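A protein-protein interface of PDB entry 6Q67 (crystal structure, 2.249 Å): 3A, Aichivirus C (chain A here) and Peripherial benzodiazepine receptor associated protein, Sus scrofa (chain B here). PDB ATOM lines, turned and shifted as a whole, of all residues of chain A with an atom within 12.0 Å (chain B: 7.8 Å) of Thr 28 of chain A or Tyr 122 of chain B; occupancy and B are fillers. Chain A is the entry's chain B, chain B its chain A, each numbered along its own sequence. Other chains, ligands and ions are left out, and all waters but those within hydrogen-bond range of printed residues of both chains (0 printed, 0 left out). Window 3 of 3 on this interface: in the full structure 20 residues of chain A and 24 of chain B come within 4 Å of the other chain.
The backbone carbonyl oxygen (O) of Met 12 of chain B lies within hydrogen-bond range of the backbone NH (N) of Val 26 of chain A, 3.0 Å away. NH1 of Arg 124 of chain B sits at hydrogen-bond distance from OG1 of Thr 28 of chain A, at 3.4 Å.
The backbone carbonyl oxygen (O) of Ile 65 of chain B sits at hydrogen-bond distance from the backbone NH (N) of Arg 124 of chain B (2.9 Å). The backbone carbonyl oxygen (O) of Tyr 122 of chain B is in hydrogen-bond range of the backbone NH (N) of Phe 67 of chain B (2.9 Å). The guanidinium group (NH2) of Arg 124 of chain B is in hydrogen-bond range of the backbone carbonyl oxygen (O) of Pro 120 of chain B, 3.1 Å away. The backbone carbonyl oxygen (O) of Tyr 122 of chain B lies within hydrogen-bond range of the guanidinium group (NE) of Arg 124 of chain B (3.2 Å). SG of Cys 126 of chain B is in hydrogen-bond range of O of Arg 124 of chain B (3.6 Å).
Among the printed residues, merely in contact across the chains: Thr 28 of chain A with Tyr 122 of chain B, Thr 28 of chain A with Pro 120 of chain B, Pro 25 of chain A with Met 12 of chain B and Thr 28 of chain A with Met 12 of chain B.
Thr 28 of chain A touches just these residues of chain B: Met 12 (3.8 Å), Pro 120 (3.7 Å), Tyr 122 (3.3 Å) and Arg 124 (3.4 Å). Of chain A, only Thr 28 comes within 4 Å of Tyr 122 of chain B. Of chain A, only Pro 25, Val 26 and Thr 28 come within 4 Å of Met 12 of chain B. No residue of chain A comes within 4 Å of Gly 66 of chain B. No residue of chain A comes within 4 Å of Gly 68 of chain B. No residue of chain A comes within 4 Å of Val 119 of chain B. Pro 120 of chain B touches just one residue of chain A: Thr 28. No residue of chain A comes within 4 Å of Val 121 of chain B. Of the printed residues of chain B, Pro 25 of chain A touches Met 12. Printed residues of chain B within 4 Å of Val 26 of chain A: Met 12. Val 69 of chain B touches none of the printed residues of chain A. Ile 65 of chain B touches none of the printed residues of chain A. The nearest residue of chain A that does not touch Tyr 122 of chain B is Ser 27 of chain A (6.5 Å).
Of the 5 printed residues of chain A, 3 touch a printed residue of chain B. Printed residues of chain A that touch a printed residue of chain B: Pro 25, Val 26 and Thr 28. Along chain A the printed residues that touch a printed residue of chain B span positions 25 to 28. Printed residues of chain B that touch a printed residue of chain A: Met 12, Pro 120, Tyr 122 and Arg 124. Along chain B the printed residues that touch a printed residue of chain A span positions 12 to 124. Among the printed residues, 6 pairs touch across the chains.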
ATOM      1  N   LYS A  24      22.514 -30.061  44.138  1.00  0.00           N
ATOM      2  CA  LYS A  24      22.674 -28.617  44.223  1.00  0.00           C
ATOM      3  C   LYS A  24      22.251 -28.026  42.877  1.00  0.00           C
ATOM      4  O   LYS A  24      22.597 -28.577  41.832  1.00  0.00           O
ATOM      5  CB  LYS A  24      24.120 -28.246  44.558  1.00  0.00           C
ATOM      6  N   PRO A  25      21.510 -26.902  42.889  1.00  0.00           N
ATOM      7  CA  PRO A  25      21.044 -26.378  41.597  1.00  0.00           C
ATOM      8  C   PRO A  25      22.137 -25.727  40.727  1.00  0.00           C
ATOM      9  O   PRO A  25      23.287 -25.599  41.153  1.00  0.00           O
ATOM     10  CB  PRO A  25      19.993 -25.331  42.006  1.00  0.00           C
ATOM     11  CG  PRO A  25      19.550 -25.731  43.367  1.00  0.00           C
ATOM     12  CD  PRO A  25      20.768 -26.306  44.020  1.00  0.00           C
ATOM     13  N   VAL A  26      21.744 -25.317  39.519  1.00  0.00           N
ATOM     14  CA  VAL A  26      22.628 -24.667  38.542  1.00  0.00           C
ATOM     15  C   VAL A  26      21.809 -23.752  37.633  1.00  0.00           C
ATOM     16  O   VAL A  26      20.655 -24.054  37.322  1.00  0.00           O
ATOM     17  CB  VAL A  26      23.388 -25.698  37.658  1.00  0.00           C
ATOM     18  CG1 VAL A  26      24.048 -25.029  36.453  1.00  0.00           C
ATOM     19  CG2 VAL A  26      24.437 -26.412  38.461  1.00  0.00           C
ATOM     20  N   SER A  27      22.416 -22.653  37.188  1.00  0.00           N
ATOM     21  CA  SER A  27      21.775 -21.745  36.234  1.00  0.00           C
ATOM     22  C   SER A  27      22.689 -21.567  35.034  1.00  0.00           C
ATOM     23  O   SER A  27      23.856 -21.964  35.069  1.00  0.00           O
ATOM     24  CB  SER A  27      21.451 -20.383  36.870  1.00  0.00           C
ATOM     25  OG  SER A  27      20.598 -20.540  37.998  1.00  0.00           O
ATOM     26  N   THR A  28      22.142 -20.996  33.967  1.00  0.00           N
ATOM     27  CA  THR A  28      22.894 -20.782  32.739  1.00  0.00           C
ATOM     28  C   THR A  28      22.500 -19.464  32.077  1.00  0.00           C
ATOM     29  O   THR A  28      23.276 -18.873  31.331  1.00  0.00           O
ATOM     30  CB  THR A  28      22.669 -21.939  31.742  1.00  0.00           C
ATOM     31  OG1 THR A  28      22.748 -23.192  32.435  1.00  0.00           O
ATOM     32  CG2 THR A  28      23.687 -21.903  30.654  1.00  0.00           C
ATOM     33  N   PRO B  10      14.509 -25.229  31.037  1.00  0.00           N
ATOM     34  CA  PRO B  10      15.028 -26.495  31.546  1.00  0.00           C
ATOM     35  C   PRO B  10      15.376 -26.375  33.008  1.00  0.00           C
ATOM     36  O   PRO B  10      15.450 -25.260  33.520  1.00  0.00           O
ATOM     37  CB  PRO B  10      16.279 -26.722  30.713  1.00  0.00           C
ATOM     38  CG  PRO B  10      16.785 -25.343  30.481  1.00  0.00           C
ATOM     39  CD  PRO B  10      15.560 -24.458  30.351  1.00  0.00           C
ATOM     40  N   MET B  12      18.357 -27.718  35.760  1.00  0.00           N
ATOM     41  CA  MET B  12      19.702 -28.282  35.818  1.00  0.00           C
ATOM     42  C   MET B  12      20.251 -28.199  37.232  1.00  0.00           C
ATOM     43  O   MET B  12      20.061 -27.198  37.921  1.00  0.00           O
ATOM     44  CB  MET B  12      20.649 -27.538  34.870  1.00  0.00           C
ATOM     45  CG  MET B  12      20.292 -27.633  33.390  1.00  0.00           C
ATOM     46  SD  MET B  12      21.528 -26.812  32.360  1.00  0.00           S
ATOM     47  CE  MET B  12      23.009 -27.736  32.786  1.00  0.00           C
ATOM     48  N   PHE B  58      25.334 -36.554  33.066  1.00  0.00           N
ATOM     49  CA  PHE B  58      26.635 -36.808  32.445  1.00  0.00           C
ATOM     50  C   PHE B  58      27.830 -36.354  33.280  1.00  0.00           C
ATOM     51  O   PHE B  58      27.715 -35.492  34.145  1.00  0.00           O
ATOM     52  CB  PHE B  58      26.717 -36.133  31.053  1.00  0.00           C
ATOM     53  CG  PHE B  58      26.769 -34.633  31.100  1.00  0.00           C
ATOM     54  CD1 PHE B  58      25.609 -33.884  31.198  1.00  0.00           C
ATOM     55  CD2 PHE B  58      27.982 -33.964  31.021  1.00  0.00           C
ATOM     56  CE1 PHE B  58      25.658 -32.490  31.225  1.00  0.00           C
ATOM     57  CE2 PHE B  58      28.038 -32.577  31.055  1.00  0.00           C
ATOM     58  CZ  PHE B  58      26.874 -31.838  31.157  1.00  0.00           C
ATOM     59  N   ASP B  64      37.109 -30.446  31.756  1.00  0.00           N
ATOM     60  CA  ASP B  64      35.745 -30.018  31.505  1.00  0.00           C
ATOM     61  C   ASP B  64      35.359 -30.385  30.081  1.00  0.00           C
ATOM     62  O   ASP B  64      36.136 -30.997  29.351  1.00  0.00           O
ATOM     63  CB  ASP B  64      35.557 -28.513  31.748  1.00  0.00           C
ATOM     64  CG  ASP B  64      36.390 -27.645  30.822  1.00  0.00           C
ATOM     65  OD1 ASP B  64      36.392 -26.416  31.035  1.00  0.00           O
ATOM     66  OD2 ASP B  64      37.035 -28.172  29.894  1.00  0.00           O
ATOM     67  N   ILE B  65      34.129 -30.060  29.718  1.00  0.00           N
ATOM     68  CA  ILE B  65      33.680 -30.155  28.341  1.00  0.00           C
ATOM     69  C   ILE B  65      32.521 -29.196  28.183  1.00  0.00           C
ATOM     70  O   ILE B  65      31.813 -28.907  29.156  1.00  0.00           O
ATOM     71  CB  ILE B  65      33.240 -31.574  27.970  1.00  0.00           C
ATOM     72  CG1 ILE B  65      33.146 -31.723  26.446  1.00  0.00           C
ATOM     73  CG2 ILE B  65      31.914 -31.909  28.671  1.00  0.00           C
ATOM     74  CD1 ILE B  65      32.902 -33.164  26.004  1.00  0.00           C
ATOM     75  N   GLY B  66      32.329 -28.699  26.965  1.00  0.00           N
ATOM     76  CA  GLY B  66      31.172 -27.882  26.672  1.00  0.00           C
ATOM     77  C   GLY B  66      29.947 -28.765  26.569  1.00  0.00           C
ATOM     78  O   GLY B  66      30.008 -29.822  25.942  1.00  0.00           O
ATOM     79  N   PHE B  67      28.842 -28.345  27.182  1.00  0.00           N
ATOM     80  CA  PHE B  67      27.581 -29.081  27.076  1.00  0.00           C
ATOM     81  C   PHE B  67      26.432 -28.145  26.776  1.00  0.00           C
ATOM     82  O   PHE B  67      26.337 -27.062  27.351  1.00  0.00           O
ATOM     83  CB  PHE B  67      27.272 -29.843  28.362  1.00  0.00           C
ATOM     84  CG  PHE B  67      25.893 -30.432  28.394  1.00  0.00           C
ATOM     85  CD1 PHE B  67      25.634 -31.645  27.774  1.00  0.00           C
ATOM     86  CD2 PHE B  67      24.858 -29.785  29.053  1.00  0.00           C
ATOM     87  CE1 PHE B  67      24.376 -32.194  27.799  1.00  0.00           C
ATOM     88  CE2 PHE B  67      23.597 -30.339  29.096  1.00  0.00           C
ATOM     89  CZ  PHE B  67      23.353 -31.543  28.471  1.00  0.00           C
ATOM     90  N   GLY B  68      25.547 -28.579  25.888  1.00  0.00           N
ATOM     91  CA  GLY B  68      24.375 -27.793  25.549  1.00  0.00           C
ATOM     92  C   GLY B  68      23.289 -28.657  24.949  1.00  0.00           C
ATOM     93  O   GLY B  68      23.511 -29.825  24.651  1.00  0.00           O
ATOM     94  N   VAL B  69      22.116 -28.071  24.755  1.00  0.00           N
ATOM     95  CA  VAL B  69      20.973 -28.837  24.296  1.00  0.00           C
ATOM     96  C   VAL B  69      20.090 -28.055  23.356  1.00  0.00           C
ATOM     97  O   VAL B  69      19.740 -26.899  23.618  1.00  0.00           O
ATOM     98  CB  VAL B  69      20.086 -29.316  25.483  1.00  0.00           C
ATOM     99  CG1 VAL B  69      19.016 -30.254  24.986  1.00  0.00           C
ATOM    100  CG2 VAL B  69      20.917 -30.016  26.542  1.00  0.00           C
ATOM    101  N   GLU B 117      16.798 -23.545  21.322  1.00  0.00           N
ATOM    102  CA  GLU B 117      17.944 -23.683  22.192  1.00  0.00           C
ATOM    103  C   GLU B 117      17.437 -23.894  23.611  1.00  0.00           C
ATOM    104  O   GLU B 117      17.027 -22.951  24.286  1.00  0.00           O
ATOM    105  CB  GLU B 117      18.830 -22.429  22.104  1.00  0.00           C
ATOM    106  CG  GLU B 117      20.172 -22.571  22.775  1.00  0.00           C
ATOM    107  CD  GLU B 117      20.969 -21.302  22.774  1.00  0.00           C
ATOM    108  OE1 GLU B 117      20.376 -20.233  23.021  1.00  0.00           O
ATOM    109  OE2 GLU B 117      22.192 -21.379  22.523  1.00  0.00           O
ATOM    110  N   ILE B 118      17.499 -25.136  24.072  1.00  0.00           N
ATOM    111  CA  ILE B 118      17.048 -25.464  25.420  1.00  0.00           C
ATOM    112  C   ILE B 118      18.110 -25.072  26.440  1.00  0.00           C
ATOM    113  O   ILE B 118      17.856 -24.267  27.340  1.00  0.00           O
ATOM    114  CB  ILE B 118      16.740 -26.943  25.528  1.00  0.00           C
ATOM    115  CG1 ILE B 118      15.903 -27.380  24.322  1.00  0.00           C
ATOM    116  CG2 ILE B 118      16.013 -27.244  26.832  1.00  0.00           C
ATOM    117  CD1 ILE B 118      14.654 -26.543  24.098  1.00  0.00           C
ATOM    118  N   VAL B 119      19.326 -25.576  26.237  1.00  0.00           N
ATOM    119  CA  VAL B 119      20.439 -25.213  27.092  1.00  0.00           C
ATOM    120  C   VAL B 119      21.551 -24.661  26.226  1.00  0.00           C
ATOM    121  O   VAL B 119      21.962 -25.302  25.254  1.00  0.00           O
ATOM    122  CB  VAL B 119      20.951 -26.437  27.891  1.00  0.00           C
ATOM    123  CG1 VAL B 119      22.178 -26.064  28.752  1.00  0.00           C
ATOM    124  CG2 VAL B 119      19.798 -27.023  28.734  1.00  0.00           C
ATOM    125  N   PRO B 120      22.113 -23.513  26.622  1.00  0.00           N
ATOM    126  CA  PRO B 120      23.178 -22.965  25.783  1.00  0.00           C
ATOM    127  C   PRO B 120      24.441 -23.770  25.959  1.00  0.00           C
ATOM    128  O   PRO B 120      24.678 -24.267  27.057  1.00  0.00           O
ATOM    129  CB  PRO B 120      23.363 -21.538  26.312  1.00  0.00           C
ATOM    130  CG  PRO B 120      22.160 -21.242  27.104  1.00  0.00           C
ATOM    131  CD  PRO B 120      21.669 -22.545  27.639  1.00  0.00           C
ATOM    132  N   VAL B 121      25.237 -23.906  24.908  1.00  0.00           N
ATOM    133  CA  VAL B 121      26.510 -24.593  25.040  1.00  0.00           C
ATOM    134  C   VAL B 121      27.460 -23.730  25.873  1.00  0.00           C
ATOM    135  O   VAL B 121      27.711 -22.568  25.561  1.00  0.00           O
ATOM    136  CB  VAL B 121      27.115 -24.914  23.671  1.00  0.00           C
ATOM    137  CG1 VAL B 121      28.485 -25.541  23.820  1.00  0.00           C
ATOM    138  CG2 VAL B 121      26.196 -25.846  22.906  1.00  0.00           C
ATOM    139  N   TYR B 122      27.962 -24.322  26.949  1.00  0.00           N
ATOM    140  CA  TYR B 122      28.905 -23.679  27.860  1.00  0.00           C
ATOM    141  C   TYR B 122      29.784 -24.777  28.439  1.00  0.00           C
ATOM    142  O   TYR B 122      29.319 -25.904  28.640  1.00  0.00           O
ATOM    143  CB  TYR B 122      28.185 -22.932  28.998  1.00  0.00           C
ATOM    144  CG  TYR B 122      27.717 -21.514  28.699  1.00  0.00           C
ATOM    145  CD1 TYR B 122      28.465 -20.648  27.907  1.00  0.00           C
ATOM    146  CD2 TYR B 122      26.529 -21.035  29.238  1.00  0.00           C
ATOM    147  CE1 TYR B 122      28.031 -19.346  27.649  1.00  0.00           C
ATOM    148  CE2 TYR B 122      26.087 -19.739  28.989  1.00  0.00           C
ATOM    149  CZ  TYR B 122      26.844 -18.900  28.193  1.00  0.00           C
ATOM    150  OH  TYR B 122      26.418 -17.614  27.939  1.00  0.00           O
ATOM    151  N   ARG B 123      31.043 -24.447  28.717  1.00  0.00           N
ATOM    152  CA  ARG B 123      31.929 -25.355  29.434  1.00  0.00           C
ATOM    153  C   ARG B 123      31.436 -25.591  30.868  1.00  0.00           C
ATOM    154  O   ARG B 123      31.126 -24.656  31.609  1.00  0.00           O
ATOM    155  CB  ARG B 123      33.359 -24.818  29.427  1.00  0.00           C
ATOM    156  CG  ARG B 123      34.029 -24.960  28.053  1.00  0.00           C
ATOM    157  CD  ARG B 123      35.274 -24.118  27.905  1.00  0.00           C
ATOM    158  NE  ARG B 123      36.380 -24.592  28.727  1.00  0.00           N
ATOM    159  CZ  ARG B 123      37.649 -24.239  28.544  1.00  0.00           C
ATOM    160  NH1 ARG B 123      37.987 -23.414  27.554  1.00  0.00           N
ATOM    161  NH2 ARG B 123      38.584 -24.724  29.343  1.00  0.00           N
ATOM    162  N   ARG B 124      31.362 -26.863  31.232  1.00  0.00           N
ATOM    163  CA  ARG B 124      30.887 -27.289  32.544  1.00  0.00           C
ATOM    164  C   ARG B 124      31.960 -28.059  33.276  1.00  0.00           C
ATOM    165  O   ARG B 124      32.552 -28.957  32.678  1.00  0.00           O
ATOM    166  CB  ARG B 124      29.667 -28.192  32.398  1.00  0.00           C
ATOM    167  CG  ARG B 124      28.654 -27.742  31.390  1.00  0.00           C
ATOM    168  CD  ARG B 124      27.866 -26.558  31.885  1.00  0.00           C
ATOM    169  NE  ARG B 124      26.953 -26.090  30.846  1.00  0.00           N
ATOM    170  CZ  ARG B 124      25.967 -25.227  31.048  1.00  0.00           C
ATOM    171  NH1 ARG B 124      25.743 -24.721  32.263  1.00  0.00           N
ATOM    172  NH2 ARG B 124      25.201 -24.877  30.026  1.00  0.00           N
ATOM    173  N   ASP B 125      32.157 -27.814  34.575  1.00  0.00           N
ATOM    174  CA  ASP B 125      33.130 -28.636  35.272  1.00  0.00           C
ATOM    175  C   ASP B 125      32.375 -29.869  35.718  1.00  0.00           C
ATOM    176  O   ASP B 125      32.004 -30.015  36.888  1.00  0.00           O
ATOM    177  CB  ASP B 125      33.704 -27.910  36.504  1.00  0.00           C
ATOM    178  CG  ASP B 125      34.531 -26.691  36.152  1.00  0.00           C
ATOM    179  OD1 ASP B 125      35.356 -26.762  35.219  1.00  0.00           O
ATOM    180  OD2 ASP B 125      34.365 -25.657  36.831  1.00  0.00           O
ATOM    181  N   CYS B 126      32.301 -30.821  34.796  1.00  0.00           N
ATOM    182  CA  CYS B 126      31.638 -32.097  35.015  1.00  0.00           C
ATOM    183  C   CYS B 126      32.666 -33.196  35.227  1.00  0.00           C
ATOM    184  O   CYS B 126      32.340 -34.384  35.198  1.00  0.00           O
ATOM    185  CB  CYS B 126      30.690 -32.424  33.861  1.00  0.00           C
ATOM    186  SG  CYS B 126      31.428 -32.356  32.235  1.00  0.00           S
ATOM    187  N   TYR B 131      26.755 -33.598  36.351  1.00  0.00           N
ATOM    188  CA  TYR B 131      25.816 -32.598  35.849  1.00  0.00           C
ATOM    189  C   TYR B 131      24.579 -33.299  35.348  1.00  0.00           C
ATOM    190  O   TYR B 131      24.661 -34.403  34.808  1.00  0.00           O
ATOM    191  CB  TYR B 131      26.453 -31.746  34.736  1.00  0.00           C
ATOM    192  CG  TYR B 131      27.177 -30.541  35.289  1.00  0.00           C
ATOM    193  CD1 TYR B 131      28.375 -30.684  35.978  1.00  0.00           C
ATOM    194  CD2 TYR B 131      26.650 -29.263  35.157  1.00  0.00           C
ATOM    195  CE1 TYR B 131      29.036 -29.580  36.507  1.00  0.00           C
ATOM    196  CE2 TYR B 131      27.309 -28.154  35.681  1.00  0.00           C
ATOM    197  CZ  TYR B 131      28.501 -28.325  36.352  1.00  0.00           C
ATOM    198  OH  TYR B 131      29.156 -27.243  36.877  1.00  0.00           O
ATOM    199  N   LYS B 146      24.712 -31.709  22.840  1.00  0.00           N
ATOM    200  CA  LYS B 146      25.979 -31.331  22.251  1.00  0.00           C
ATOM    201  C   LYS B 146      27.056 -31.463  23.287  1.00  0.00           C
ATOM    202  O   LYS B 146      27.095 -30.687  24.238  1.00  0.00           O
ATOM    203  CB  LYS B 146      25.958 -29.886  21.721  1.00  0.00           C
ATOM    204  CG  LYS B 146      24.998 -29.628  20.572  1.00  0.00           C
ATOM    205  CD  LYS B 146      25.464 -30.284  19.292  1.00  0.00           C
ATOM    206  CE  LYS B 146      24.654 -29.790  18.114  1.00  0.00           C
ATOM    207  NZ  LYS B 146      25.016 -30.516  16.873  1.00  0.00           N
ATOM    208  N   ASP B 148      30.720 -30.740  23.429  1.00  0.00           N
ATOM    209  CA  ASP B 148      31.519 -29.877  22.588  1.00  0.00           C
ATOM    210  C   ASP B 148      32.946 -29.709  23.096  1.00  0.00           C
ATOM    211  O   ASP B 148      33.182 -28.967  24.045  1.00  0.00           O
ATOM    212  CB  ASP B 148      30.830 -28.518  22.515  1.00  0.00           C
ATOM    213  CG  ASP B 148      31.375 -27.635  21.402  1.00  0.00           C
ATOM    214  OD1 ASP B 148      32.597 -27.678  21.156  1.00  0.00           O
ATOM    215  OD2 ASP B 148      30.577 -26.891  20.782  1.00  0.00           O
ATOM    216  N   TYR B 151      37.232 -26.555  21.458  1.00  0.00           N
ATOM    217  CA  TYR B 151      38.241 -25.603  21.948  1.00  0.00           C
ATOM    218  C   TYR B 151      39.491 -26.295  22.478  1.00  0.00           C
ATOM    219  O   TYR B 151      40.446 -25.639  22.890  1.00  0.00           O
ATOM    220  CB  TYR B 151      37.658 -24.742  23.065  1.00  0.00           C
ATOM    221  CG  TYR B 151      37.225 -25.570  24.274  1.00  0.00           C
ATOM    222  CD1 TYR B 151      35.960 -26.146  24.330  1.00  0.00           C
ATOM    223  CD2 TYR B 151      38.082 -25.781  25.343  1.00  0.00           C
ATOM    224  CE1 TYR B 151      35.554 -26.905  25.419  1.00  0.00           C
ATOM    225  CE2 TYR B 151      37.686 -26.547  26.442  1.00  0.00           C
ATOM    226  CZ  TYR B 151      36.415 -27.105  26.471  1.00  0.00           C
ATOM    227  OH  TYR B 151      36.000 -27.866  27.542  1.00  0.00           O
